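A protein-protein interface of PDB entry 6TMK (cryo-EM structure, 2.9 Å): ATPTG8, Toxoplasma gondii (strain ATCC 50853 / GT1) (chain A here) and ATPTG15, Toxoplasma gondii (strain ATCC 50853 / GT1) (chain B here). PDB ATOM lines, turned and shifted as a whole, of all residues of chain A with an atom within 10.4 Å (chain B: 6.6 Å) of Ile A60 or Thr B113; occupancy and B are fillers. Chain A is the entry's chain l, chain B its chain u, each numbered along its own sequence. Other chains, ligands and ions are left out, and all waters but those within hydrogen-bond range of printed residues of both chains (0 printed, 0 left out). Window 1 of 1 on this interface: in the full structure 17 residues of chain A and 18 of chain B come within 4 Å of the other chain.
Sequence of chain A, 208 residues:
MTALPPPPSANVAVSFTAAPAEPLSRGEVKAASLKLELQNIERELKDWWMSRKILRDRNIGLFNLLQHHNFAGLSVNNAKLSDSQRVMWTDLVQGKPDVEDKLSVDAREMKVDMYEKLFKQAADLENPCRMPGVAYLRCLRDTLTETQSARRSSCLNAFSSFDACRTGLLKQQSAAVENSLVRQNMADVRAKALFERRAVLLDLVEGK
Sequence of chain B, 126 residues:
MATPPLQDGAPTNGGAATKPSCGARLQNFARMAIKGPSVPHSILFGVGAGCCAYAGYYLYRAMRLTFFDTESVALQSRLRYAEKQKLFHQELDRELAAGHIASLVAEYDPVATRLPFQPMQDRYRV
O of Ile A60 lies within hydrogen-bond range of ND2 of Asn A64 (3.3 Å). OD2 of Asp B109 lies close to N of Val B111 (3.3 Å). OG1 of Thr B113 sits at hydrogen-bond distance from O of Pro B110. The side-chain carboxylate (OD2) of Asp A188 is in salt-bridge range of the guanidinium group (NH2) of Arg A52. The guanidinium group of Arg A52 lies close to the side-chain amide oxygen of Gln A184 (3.3 Å). OD1 of Asn A59 lies close to O of Leu A55 (2.6 Å).
Leu B115 touches Arg A52. Arg A56 touches Ala B112. O of Asn A59 touches CE1 of Tyr B108, at 3.3 Å. OD1 of Asn A59 touches CB of Ala B112 (2.9 Å). Ile A60 touches Thr B113. CB of Phe A63 touches OH of Tyr B108 (3.8 Å). Phe A63 touches Tyr B124. CG2 of Val B111 touches O of Val A177, at 3.9 Å. CD of Arg B114 touches CD2 of Leu A181, at 3.6 Å. CA of Ala B112 touches NE2 of Gln A184, at 3.7 Å.
Of the printed residues of chain B, Arg A52 touches Arg B114 (2.6 Å) and Leu B115 (3.5 Å). Of the printed residues of chain B, Ile A60 touches Thr B113 (3.9 Å). Of the printed residues of chain B, Gln A184 touches Val B111, Ala B112 and Arg B114. Printed residues of chain A within 4 Å of Tyr B108: Asn A59 (3.3 Å), Leu A62 (3.9 Å) and Phe A63 (3.8 Å). Of the printed residues of chain A, Asp B109 touches Asn A59 and Ser A180. Of chain A, only Arg A56 (2.3 Å) and Ile A60 (3.9 Å) come within 4 Å of Thr B113. Tyr B124 touches one residue of chain A. The nearest residue of chain B that does not touch Ile A60 is Tyr B124 (4.3 Å). The nearest printed residue of chain B that does not touch Arg A52 is Ala B112 (4.6 Å).
The side-chain amide nitrogen of Asn A59 lies close to the backbone NH of Asp B109 (3.4 Å). The backbone carbonyl oxygen (O) of Thr B113 sits close to the guanidinium group (NH1) of Arg A56 (2.3 Å). NH1 of Arg A52 sits at hydrogen-bond distance from O of Arg B114. The guanidinium group (NH2) of Arg B114 lies within salt-bridge range of the side-chain carboxylate (OD2) of Asp A188 (3.8 Å). The side-chain amide oxygen of Gln A184 is in hydrogen-bond range of the guanidinium group of Arg B114, at 2.4 Å. The side-chain hydroxyl of Ser A180 is in hydrogen-bond range of the side-chain carboxylate of Asp B109, at 3.4 Å. The side-chain amide nitrogen (NE2) of Gln A184 is in hydrogen-bond range of the backbone carbonyl oxygen (O) of Val B111, 2.9 Å away.
Of the 11 printed residues of chain B, 8 touch a printed residue of chain A. Printed residues of chain B that touch a printed residue of chain A: Tyr B108, Asp B109, Val B111, Ala B112, Thr B113, Arg B114, Leu B115 and Tyr B124. Among the printed residues, 19 pairs touch across the chains.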
ATOM      1  N   SER A  51      11.949  39.586 -14.098  1.00  0.00           N
ATOM      2  CA  SER A  51      10.740  39.234 -14.828  1.00  0.00           C
ATOM      3  C   SER A  51      10.781  37.777 -15.264  1.00  0.00           C
ATOM      4  O   SER A  51       9.804  37.035 -15.098  1.00  0.00           O
ATOM      5  CB  SER A  51      10.574  40.162 -16.028  1.00  0.00           C
ATOM      6  OG  SER A  51      10.772  41.512 -15.660  1.00  0.00           O
ATOM      7  N   ARG A  52      11.921  37.344 -15.802  1.00  0.00           N
ATOM      8  CA  ARG A  52      12.062  35.969 -16.259  1.00  0.00           C
ATOM      9  C   ARG A  52      11.875  34.990 -15.107  1.00  0.00           C
ATOM     10  O   ARG A  52      11.147  33.997 -15.229  1.00  0.00           O
ATOM     11  CB  ARG A  52      13.435  35.807 -16.909  1.00  0.00           C
ATOM     12  CG  ARG A  52      13.672  34.524 -17.651  1.00  0.00           C
ATOM     13  CD  ARG A  52      12.901  34.467 -18.944  1.00  0.00           C
ATOM     14  NE  ARG A  52      12.965  33.140 -19.545  1.00  0.00           N
ATOM     15  CZ  ARG A  52      13.605  32.840 -20.666  1.00  0.00           C
ATOM     16  NH1 ARG A  52      13.592  31.599 -21.108  1.00  0.00           N
ATOM     17  NH2 ARG A  52      14.254  33.763 -21.352  1.00  0.00           N
ATOM     18  N   LYS A  53      12.520  35.265 -13.976  1.00  0.00           N
ATOM     19  CA  LYS A  53      12.426  34.391 -12.814  1.00  0.00           C
ATOM     20  C   LYS A  53      10.991  34.290 -12.310  1.00  0.00           C
ATOM     21  O   LYS A  53      10.483  33.191 -12.050  1.00  0.00           O
ATOM     22  CB  LYS A  53      13.359  34.921 -11.728  1.00  0.00           C
ATOM     23  CG  LYS A  53      13.427  34.124 -10.465  1.00  0.00           C
ATOM     24  CD  LYS A  53      14.267  32.906 -10.650  1.00  0.00           C
ATOM     25  CE  LYS A  53      14.233  32.030  -9.431  1.00  0.00           C
ATOM     26  NZ  LYS A  53      14.999  32.641  -8.342  1.00  0.00           N
ATOM     27  N   ILE A  54      10.323  35.436 -12.151  1.00  0.00           N
ATOM     28  CA  ILE A  54       8.971  35.429 -11.608  1.00  0.00           C
ATOM     29  C   ILE A  54       8.032  34.677 -12.534  1.00  0.00           C
ATOM     30  O   ILE A  54       7.196  33.885 -12.083  1.00  0.00           O
ATOM     31  CB  ILE A  54       8.482  36.865 -11.349  1.00  0.00           C
ATOM     32  CG1 ILE A  54       9.311  37.520 -10.258  1.00  0.00           C
ATOM     33  CG2 ILE A  54       7.043  36.862 -10.915  1.00  0.00           C
ATOM     34  CD1 ILE A  54       9.296  38.994 -10.315  1.00  0.00           C
ATOM     35  N   LEU A  55       8.138  34.919 -13.841  1.00  0.00           N
ATOM     36  CA  LEU A  55       7.244  34.249 -14.775  1.00  0.00           C
ATOM     37  C   LEU A  55       7.493  32.748 -14.805  1.00  0.00           C
ATOM     38  O   LEU A  55       6.542  31.960 -14.833  1.00  0.00           O
ATOM     39  CB  LEU A  55       7.401  34.856 -16.163  1.00  0.00           C
ATOM     40  CG  LEU A  55       6.622  36.147 -16.369  1.00  0.00           C
ATOM     41  CD1 LEU A  55       7.095  36.843 -17.606  1.00  0.00           C
ATOM     42  CD2 LEU A  55       5.144  35.873 -16.459  1.00  0.00           C
ATOM     43  N   ARG A  56       8.759  32.332 -14.795  1.00  0.00           N
ATOM     44  CA  ARG A  56       9.068  30.909 -14.747  1.00  0.00           C
ATOM     45  C   ARG A  56       8.447  30.256 -13.523  1.00  0.00           C
ATOM     46  O   ARG A  56       7.791  29.212 -13.623  1.00  0.00           O
ATOM     47  CB  ARG A  56      10.577  30.711 -14.755  1.00  0.00           C
ATOM     48  CG  ARG A  56      11.021  29.339 -15.179  1.00  0.00           C
ATOM     49  CD  ARG A  56      12.504  29.185 -15.025  1.00  0.00           C
ATOM     50  NE  ARG A  56      12.882  27.842 -14.605  1.00  0.00           N
ATOM     51  CZ  ARG A  56      12.791  26.771 -15.379  1.00  0.00           C
ATOM     52  NH1 ARG A  56      12.338  26.884 -16.615  1.00  0.00           N
ATOM     53  NH2 ARG A  56      13.155  25.593 -14.911  1.00  0.00           N
ATOM     54  N   ASP A  57       8.637  30.866 -12.354  1.00  0.00           N
ATOM     55  CA  ASP A  57       8.110  30.287 -11.124  1.00  0.00           C
ATOM     56  C   ASP A  57       6.589  30.222 -11.156  1.00  0.00           C
ATOM     57  O   ASP A  57       5.993  29.191 -10.815  1.00  0.00           O
ATOM     58  CB  ASP A  57       8.601  31.087  -9.922  1.00  0.00           C
ATOM     59  CG  ASP A  57      10.073  30.869  -9.640  1.00  0.00           C
ATOM     60  OD1 ASP A  57      10.745  30.200 -10.452  1.00  0.00           O
ATOM     61  OD2 ASP A  57      10.560  31.358  -8.598  1.00  0.00           O
ATOM     62  N   ARG A  58       5.941  31.307 -11.575  1.00  0.00           N
ATOM     63  CA  ARG A  58       4.486  31.330 -11.616  1.00  0.00           C
ATOM     64  C   ARG A  58       3.950  30.257 -12.549  1.00  0.00           C
ATOM     65  O   ARG A  58       2.996  29.546 -12.214  1.00  0.00           O
ATOM     66  CB  ARG A  58       3.993  32.703 -12.056  1.00  0.00           C
ATOM     67  CG  ARG A  58       2.510  32.751 -12.331  1.00  0.00           C
ATOM     68  CD  ARG A  58       2.015  34.142 -12.574  1.00  0.00           C
ATOM     69  NE  ARG A  58       0.613  34.140 -12.962  1.00  0.00           N
ATOM     70  CZ  ARG A  58      -0.397  34.038 -12.110  1.00  0.00           C
ATOM     71  NH1 ARG A  58      -0.174  33.939 -10.816  1.00  0.00           N
ATOM     72  NH2 ARG A  58      -1.636  34.035 -12.552  1.00  0.00           N
ATOM     73  N   ASN A  59       4.539  30.132 -13.737  1.00  0.00           N
ATOM     74  CA  ASN A  59       3.977  29.219 -14.717  1.00  0.00           C
ATOM     75  C   ASN A  59       4.265  27.770 -14.358  1.00  0.00           C
ATOM     76  O   ASN A  59       3.435  26.893 -14.624  1.00  0.00           O
ATOM     77  CB  ASN A  59       4.523  29.562 -16.096  1.00  0.00           C
ATOM     78  CG  ASN A  59       4.070  30.921 -16.566  1.00  0.00           C
ATOM     79  OD1 ASN A  59       4.880  31.802 -16.836  1.00  0.00           O
ATOM     80  ND2 ASN A  59       2.770  31.106 -16.644  1.00  0.00           N
ATOM     81  N   ILE A  60       5.398  27.495 -13.715  1.00  0.00           N
ATOM     82  CA  ILE A  60       5.627  26.146 -13.217  1.00  0.00           C
ATOM     83  C   ILE A  60       4.644  25.817 -12.103  1.00  0.00           C
ATOM     84  O   ILE A  60       4.151  24.688 -12.008  1.00  0.00           O
ATOM     85  CB  ILE A  60       7.087  25.977 -12.767  1.00  0.00           C
ATOM     86  CG1 ILE A  60       7.982  25.774 -13.983  1.00  0.00           C
ATOM     87  CG2 ILE A  60       7.222  24.804 -11.844  1.00  0.00           C
ATOM     88  CD1 ILE A  60       9.391  26.140 -13.763  1.00  0.00           C
ATOM     89  N   GLY A  61       4.339  26.791 -11.247  1.00  0.00           N
ATOM     90  CA  GLY A  61       3.343  26.557 -10.219  1.00  0.00           C
ATOM     91  C   GLY A  61       1.968  26.279 -10.791  1.00  0.00           C
ATOM     92  O   GLY A  61       1.253  25.400 -10.310  1.00  0.00           O
ATOM     93  N   LEU A  62       1.575  27.028 -11.821  1.00  0.00           N
ATOM     94  CA  LEU A  62       0.314  26.750 -12.502  1.00  0.00           C
ATOM     95  C   LEU A  62       0.304  25.356 -13.105  1.00  0.00           C
ATOM     96  O   LEU A  62      -0.694  24.635 -13.011  1.00  0.00           O
ATOM     97  CB  LEU A  62       0.031  27.789 -13.581  1.00  0.00           C
ATOM     98  CG  LEU A  62      -0.365  29.187 -13.155  1.00  0.00           C
ATOM     99  CD1 LEU A  62      -0.415  30.093 -14.340  1.00  0.00           C
ATOM    100  CD2 LEU A  62      -1.731  29.103 -12.536  1.00  0.00           C
ATOM    101  N   PHE A  63       1.391  24.971 -13.771  1.00  0.00           N
ATOM    102  CA  PHE A  63       1.447  23.640 -14.353  1.00  0.00           C
ATOM    103  C   PHE A  63       1.290  22.571 -13.286  1.00  0.00           C
ATOM    104  O   PHE A  63       0.547  21.601 -13.472  1.00  0.00           O
ATOM    105  CB  PHE A  63       2.760  23.443 -15.098  1.00  0.00           C
ATOM    106  CG  PHE A  63       2.994  22.032 -15.527  1.00  0.00           C
ATOM    107  CD1 PHE A  63       2.326  21.511 -16.612  1.00  0.00           C
ATOM    108  CD2 PHE A  63       3.868  21.223 -14.837  1.00  0.00           C
ATOM    109  CE1 PHE A  63       2.533  20.223 -17.005  1.00  0.00           C
ATOM    110  CE2 PHE A  63       4.078  19.931 -15.231  1.00  0.00           C
ATOM    111  CZ  PHE A  63       3.407  19.429 -16.314  1.00  0.00           C
ATOM    112  N   ASN A  64       1.977  22.730 -12.157  1.00  0.00           N
ATOM    113  CA  ASN A  64       1.885  21.733 -11.100  1.00  0.00           C
ATOM    114  C   ASN A  64       0.492  21.700 -10.497  1.00  0.00           C
ATOM    115  O   ASN A  64      -0.020  20.629 -10.166  1.00  0.00           O
ATOM    116  CB  ASN A  64       2.925  22.025 -10.029  1.00  0.00           C
ATOM    117  CG  ASN A  64       4.312  21.604 -10.439  1.00  0.00           C
ATOM    118  OD1 ASN A  64       4.495  20.620 -11.153  1.00  0.00           O
ATOM    119  ND2 ASN A  64       5.300  22.350  -9.991  1.00  0.00           N
ATOM    120  N   LEU A  65      -0.149  22.858 -10.375  1.00  0.00           N
ATOM    121  CA  LEU A  65      -1.512  22.906  -9.863  1.00  0.00           C
ATOM    122  C   LEU A  65      -2.482  22.199 -10.802  1.00  0.00           C
ATOM    123  O   LEU A  65      -3.356  21.443 -10.356  1.00  0.00           O
ATOM    124  CB  LEU A  65      -1.917  24.359  -9.665  1.00  0.00           C
ATOM    125  CG  LEU A  65      -3.324  24.659  -9.184  1.00  0.00           C
ATOM    126  CD1 LEU A  65      -3.482  24.156  -7.786  1.00  0.00           C
ATOM    127  CD2 LEU A  65      -3.588  26.136  -9.256  1.00  0.00           C
ATOM    128  N   LEU A  66      -2.362  22.454 -12.104  1.00  0.00           N
ATOM    129  CA  LEU A  66      -3.252  21.824 -13.071  1.00  0.00           C
ATOM    130  C   LEU A  66      -3.012  20.323 -13.148  1.00  0.00           C
ATOM    131  O   LEU A  66      -3.959  19.545 -13.296  1.00  0.00           O
ATOM    132  CB  LEU A  66      -3.061  22.464 -14.442  1.00  0.00           C
ATOM    133  CG  LEU A  66      -3.328  23.961 -14.532  1.00  0.00           C
ATOM    134  CD1 LEU A  66      -2.657  24.532 -15.755  1.00  0.00           C
ATOM    135  CD2 LEU A  66      -4.803  24.238 -14.570  1.00  0.00           C
ATOM    136  N   GLN A  67      -1.753  19.899 -13.045  1.00  0.00           N
ATOM    137  CA  GLN A  67      -1.448  18.477 -12.991  1.00  0.00           C
ATOM    138  C   GLN A  67      -2.003  17.849 -11.722  1.00  0.00           C
ATOM    139  O   GLN A  67      -2.436  16.692 -11.734  1.00  0.00           O
ATOM    140  CB  GLN A  67       0.062  18.279 -13.086  1.00  0.00           C
ATOM    141  CG  GLN A  67       0.501  17.043 -13.821  1.00  0.00           C
ATOM    142  CD  GLN A  67       1.994  16.838 -13.754  1.00  0.00           C
ATOM    143  OE1 GLN A  67       2.639  17.208 -12.775  1.00  0.00           O
ATOM    144  NE2 GLN A  67       2.557  16.241 -14.797  1.00  0.00           N
ATOM    145  N   HIS A  68      -1.995  18.601 -10.625  1.00  0.00           N
ATOM    146  CA  HIS A  68      -2.512  18.115  -9.356  1.00  0.00           C
ATOM    147  C   HIS A  68      -4.016  17.908  -9.422  1.00  0.00           C
ATOM    148  O   HIS A  68      -4.531  16.893  -8.940  1.00  0.00           O
ATOM    149  CB  HIS A  68      -2.148  19.131  -8.276  1.00  0.00           C
ATOM    150  CG  HIS A  68      -2.562  18.749  -6.893  1.00  0.00           C
ATOM    151  ND1 HIS A  68      -3.313  19.583  -6.096  1.00  0.00           N
ATOM    152  CD2 HIS A  68      -2.293  17.656  -6.145  1.00  0.00           C
ATOM    153  CE1 HIS A  68      -3.512  19.007  -4.926  1.00  0.00           C
ATOM    154  NE2 HIS A  68      -2.903  17.837  -4.930  1.00  0.00           N
ATOM    155  N   VAL A 177       2.106  30.795 -28.716  1.00  0.00           N
ATOM    156  CA  VAL A 177       3.376  30.121 -28.458  1.00  0.00           C
ATOM    157  C   VAL A 177       4.482  30.726 -29.314  1.00  0.00           C
ATOM    158  O   VAL A 177       5.568  31.057 -28.820  1.00  0.00           O
ATOM    159  CB  VAL A 177       3.240  28.611 -28.701  1.00  0.00           C
ATOM    160  CG1 VAL A 177       4.587  27.941 -28.618  1.00  0.00           C
ATOM    161  CG2 VAL A 177       2.301  28.010 -27.702  1.00  0.00           C
ATOM    162  N   SER A 180       5.392  34.372 -28.199  1.00  0.00           N
ATOM    163  CA  SER A 180       6.087  34.375 -26.921  1.00  0.00           C
ATOM    164  C   SER A 180       7.521  33.893 -27.076  1.00  0.00           C
ATOM    165  O   SER A 180       8.440  34.456 -26.473  1.00  0.00           O
ATOM    166  CB  SER A 180       5.330  33.511 -25.920  1.00  0.00           C
ATOM    167  OG  SER A 180       4.049  34.045 -25.662  1.00  0.00           O
ATOM    168  N   LEU A 181       7.737  32.859 -27.893  1.00  0.00           N
ATOM    169  CA  LEU A 181       9.094  32.379 -28.125  1.00  0.00           C
ATOM    170  C   LEU A 181       9.959  33.467 -28.742  1.00  0.00           C
ATOM    171  O   LEU A 181      11.100  33.695 -28.317  1.00  0.00           O
ATOM    172  CB  LEU A 181       9.069  31.157 -29.034  1.00  0.00           C
ATOM    173  CG  LEU A 181       8.796  29.805 -28.394  1.00  0.00           C
ATOM    174  CD1 LEU A 181       8.616  28.777 -29.467  1.00  0.00           C
ATOM    175  CD2 LEU A 181       9.921  29.409 -27.488  1.00  0.00           C
ATOM    176  N   GLN A 184      10.710  36.256 -26.169  1.00  0.00           N
ATOM    177  CA  GLN A 184      11.651  35.745 -25.185  1.00  0.00           C
ATOM    178  C   GLN A 184      13.073  35.724 -25.732  1.00  0.00           C
ATOM    179  O   GLN A 184      14.018  36.166 -25.064  1.00  0.00           O
ATOM    180  CB  GLN A 184      11.208  34.346 -24.777  1.00  0.00           C
ATOM    181  CG  GLN A 184      11.656  33.886 -23.440  1.00  0.00           C
ATOM    182  CD  GLN A 184      11.252  32.463 -23.172  1.00  0.00           C
ATOM    183  OE1 GLN A 184      11.736  31.536 -23.816  1.00  0.00           O
ATOM    184  NE2 GLN A 184      10.349  32.280 -22.227  1.00  0.00           N
ATOM    185  N   ASP A 188      16.380  37.816 -24.397  1.00  0.00           N
ATOM    186  CA  ASP A 188      17.575  37.152 -23.888  1.00  0.00           C
ATOM    187  C   ASP A 188      18.819  37.587 -24.654  1.00  0.00           C
ATOM    188  O   ASP A 188      19.887  37.785 -24.060  1.00  0.00           O
ATOM    189  CB  ASP A 188      17.403  35.641 -23.955  1.00  0.00           C
ATOM    190  CG  ASP A 188      16.203  35.158 -23.172  1.00  0.00           C
ATOM    191  OD1 ASP A 188      15.760  35.877 -22.257  1.00  0.00           O
ATOM    192  OD2 ASP A 188      15.707  34.053 -23.466  1.00  0.00           O
ATOM    193  N   TYR B 108      -1.954  30.860 -18.237  1.00  0.00           N
ATOM    194  CA  TYR B 108      -0.820  29.952 -18.296  1.00  0.00           C
ATOM    195  C   TYR B 108      -0.077  30.099 -19.615  1.00  0.00           C
ATOM    196  O   TYR B 108      -0.668  30.015 -20.693  1.00  0.00           O
ATOM    197  CB  TYR B 108      -1.282  28.512 -18.112  1.00  0.00           C
ATOM    198  CG  TYR B 108      -0.181  27.495 -18.265  1.00  0.00           C
ATOM    199  CD1 TYR B 108       0.857  27.433 -17.358  1.00  0.00           C
ATOM    200  CD2 TYR B 108      -0.174  26.604 -19.318  1.00  0.00           C
ATOM    201  CE1 TYR B 108       1.860  26.520 -17.491  1.00  0.00           C
ATOM    202  CE2 TYR B 108       0.829  25.684 -19.458  1.00  0.00           C
ATOM    203  CZ  TYR B 108       1.845  25.645 -18.540  1.00  0.00           C
ATOM    204  OH  TYR B 108       2.852  24.725 -18.674  1.00  0.00           O
ATOM    205  N   ASP B 109       1.224  30.329 -19.515  1.00  0.00           N
ATOM    206  CA  ASP B 109       2.114  30.442 -20.666  1.00  0.00           C
ATOM    207  C   ASP B 109       3.207  29.395 -20.545  1.00  0.00           C
ATOM    208  O   ASP B 109       4.105  29.542 -19.694  1.00  0.00           O
ATOM    209  CB  ASP B 109       2.722  31.839 -20.752  1.00  0.00           C
ATOM    210  CG  ASP B 109       3.348  32.117 -22.099  1.00  0.00           C
ATOM    211  OD1 ASP B 109       3.745  33.275 -22.343  1.00  0.00           O
ATOM    212  OD2 ASP B 109       3.436  31.179 -22.919  1.00  0.00           O
ATOM    213  N   PRO B 110       3.188  28.322 -21.340  1.00  0.00           N
ATOM    214  CA  PRO B 110       4.216  27.288 -21.194  1.00  0.00           C
ATOM    215  C   PRO B 110       5.567  27.665 -21.764  1.00  0.00           C
ATOM    216  O   PRO B 110       6.529  26.909 -21.574  1.00  0.00           O
ATOM    217  CB  PRO B 110       3.612  26.110 -21.957  1.00  0.00           C
ATOM    218  CG  PRO B 110       2.817  26.745 -23.007  1.00  0.00           C
ATOM    219  CD  PRO B 110       2.196  27.944 -22.358  1.00  0.00           C
ATOM    220  N   VAL B 111       5.676  28.799 -22.452  1.00  0.00           N
ATOM    221  CA  VAL B 111       6.964  29.226 -22.977  1.00  0.00           C
ATOM    222  C   VAL B 111       7.825  29.817 -21.873  1.00  0.00           C
ATOM    223  O   VAL B 111       9.057  29.754 -21.939  1.00  0.00           O
ATOM    224  CB  VAL B 111       6.760  30.229 -24.121  1.00  0.00           C
ATOM    225  CG1 VAL B 111       8.084  30.754 -24.603  1.00  0.00           C
ATOM    226  CG2 VAL B 111       6.007  29.581 -25.249  1.00  0.00           C
ATOM    227  N   ALA B 112       7.200  30.391 -20.847  1.00  0.00           N
ATOM    228  CA  ALA B 112       7.944  30.945 -19.728  1.00  0.00           C
ATOM    229  C   ALA B 112       8.700  29.884 -18.948  1.00  0.00           C
ATOM    230  O   ALA B 112       9.674  30.210 -18.262  1.00  0.00           O
ATOM    231  CB  ALA B 112       6.988  31.676 -18.802  1.00  0.00           C
ATOM    232  N   THR B 113       8.266  28.630 -19.021  1.00  0.00           N
ATOM    233  CA  THR B 113       9.019  27.542 -18.422  1.00  0.00           C
ATOM    234  C   THR B 113      10.328  27.287 -19.147  1.00  0.00           C
ATOM    235  O   THR B 113      11.223  26.653 -18.583  1.00  0.00           O
ATOM    236  CB  THR B 113       8.174  26.272 -18.410  1.00  0.00           C
ATOM    237  OG1 THR B 113       7.894  25.864 -19.753  1.00  0.00           O
ATOM    238  CG2 THR B 113       6.878  26.517 -17.695  1.00  0.00           C
ATOM    239  N   ARG B 114      10.455  27.771 -20.376  1.00  0.00           N
ATOM    240  CA  ARG B 114      11.677  27.583 -21.137  1.00  0.00           C
ATOM    241  C   ARG B 114      12.846  28.290 -20.469  1.00  0.00           C
ATOM    242  O   ARG B 114      12.718  29.410 -19.970  1.00  0.00           O
ATOM    243  CB  ARG B 114      11.485  28.113 -22.554  1.00  0.00           C
ATOM    244  CG  ARG B 114      12.483  27.617 -23.551  1.00  0.00           C
ATOM    245  CD  ARG B 114      12.205  28.199 -24.912  1.00  0.00           C
ATOM    246  NE  ARG B 114      12.613  29.594 -25.010  1.00  0.00           N
ATOM    247  CZ  ARG B 114      13.827  29.994 -25.368  1.00  0.00           C
ATOM    248  NH1 ARG B 114      14.765  29.110 -25.660  1.00  0.00           N
ATOM    249  NH2 ARG B 114      14.104  31.285 -25.430  1.00  0.00           N
ATOM    250  N   LEU B 115      13.943  27.653 -20.470  1.00  0.00           N
ATOM    251  CA  LEU B 115      15.186  28.222 -19.988  1.00  0.00           C
ATOM    252  C   LEU B 115      15.882  28.946 -21.136  1.00  0.00           C
ATOM    253  O   LEU B 115      15.754  28.542 -22.294  1.00  0.00           O
ATOM    254  CB  LEU B 115      16.088  27.122 -19.444  1.00  0.00           C
ATOM    255  CG  LEU B 115      17.121  27.503 -18.392  1.00  0.00           C
ATOM    256  CD1 LEU B 115      16.411  27.843 -17.103  1.00  0.00           C
ATOM    257  CD2 LEU B 115      18.139  26.391 -18.184  1.00  0.00           C
ATOM    258  N   MET B 120      12.071  24.095 -25.895  1.00  0.00           N
ATOM    259  CA  MET B 120      10.864  23.942 -25.105  1.00  0.00           C
ATOM    260  C   MET B 120      10.492  22.472 -24.974  1.00  0.00           C
ATOM    261  O   MET B 120      10.692  21.671 -25.892  1.00  0.00           O
ATOM    262  CB  MET B 120       9.719  24.718 -25.745  1.00  0.00           C
ATOM    263  CG  MET B 120       8.552  24.946 -24.828  1.00  0.00           C
ATOM    264  SD  MET B 120       7.104  25.530 -25.717  1.00  0.00           S
ATOM    265  CE  MET B 120       5.844  25.072 -24.547  1.00  0.00           C
ATOM    266  N   GLN B 121       9.947  22.119 -23.815  1.00  0.00           N
ATOM    267  CA  GLN B 121       9.589  20.744 -23.508  1.00  0.00           C
ATOM    268  C   GLN B 121       8.112  20.492 -23.773  1.00  0.00           C
ATOM    269  O   GLN B 121       7.255  21.298 -23.403  1.00  0.00           O
ATOM    270  CB  GLN B 121       9.895  20.416 -22.051  1.00  0.00           C
ATOM    271  CG  GLN B 121      11.354  20.505 -21.684  1.00  0.00           C
ATOM    272  CD  GLN B 121      11.609  20.098 -20.253  1.00  0.00           C
ATOM    273  OE1 GLN B 121      11.309  18.976 -19.849  1.00  0.00           O
ATOM    274  NE2 GLN B 121      12.151  21.015 -19.470  1.00  0.00           N
ATOM    275  N   TYR B 124       5.277  20.414 -20.874  1.00  0.00           N
ATOM    276  CA  TYR B 124       4.371  21.518 -20.566  1.00  0.00           C
ATOM    277  C   TYR B 124       3.444  21.814 -21.742  1.00  0.00           C
ATOM    278  O   TYR B 124       3.244  22.960 -22.136  1.00  0.00           O
ATOM    279  CB  TYR B 124       5.176  22.751 -20.184  1.00  0.00           C
ATOM    280  CG  TYR B 124       6.142  22.548 -19.040  1.00  0.00           C
ATOM    281  CD1 TYR B 124       5.738  22.708 -17.729  1.00  0.00           C
ATOM    282  CD2 TYR B 124       7.460  22.204 -19.273  1.00  0.00           C
ATOM    283  CE1 TYR B 124       6.613  22.528 -16.687  1.00  0.00           C
ATOM    284  CE2 TYR B 124       8.341  22.023 -18.234  1.00  0.00           C
ATOM    285  CZ  TYR B 124       7.910  22.185 -16.942  1.00  0.00           C
ATOM    286  OH  TYR B 124       8.778  22.008 -15.895  1.00  0.00           O
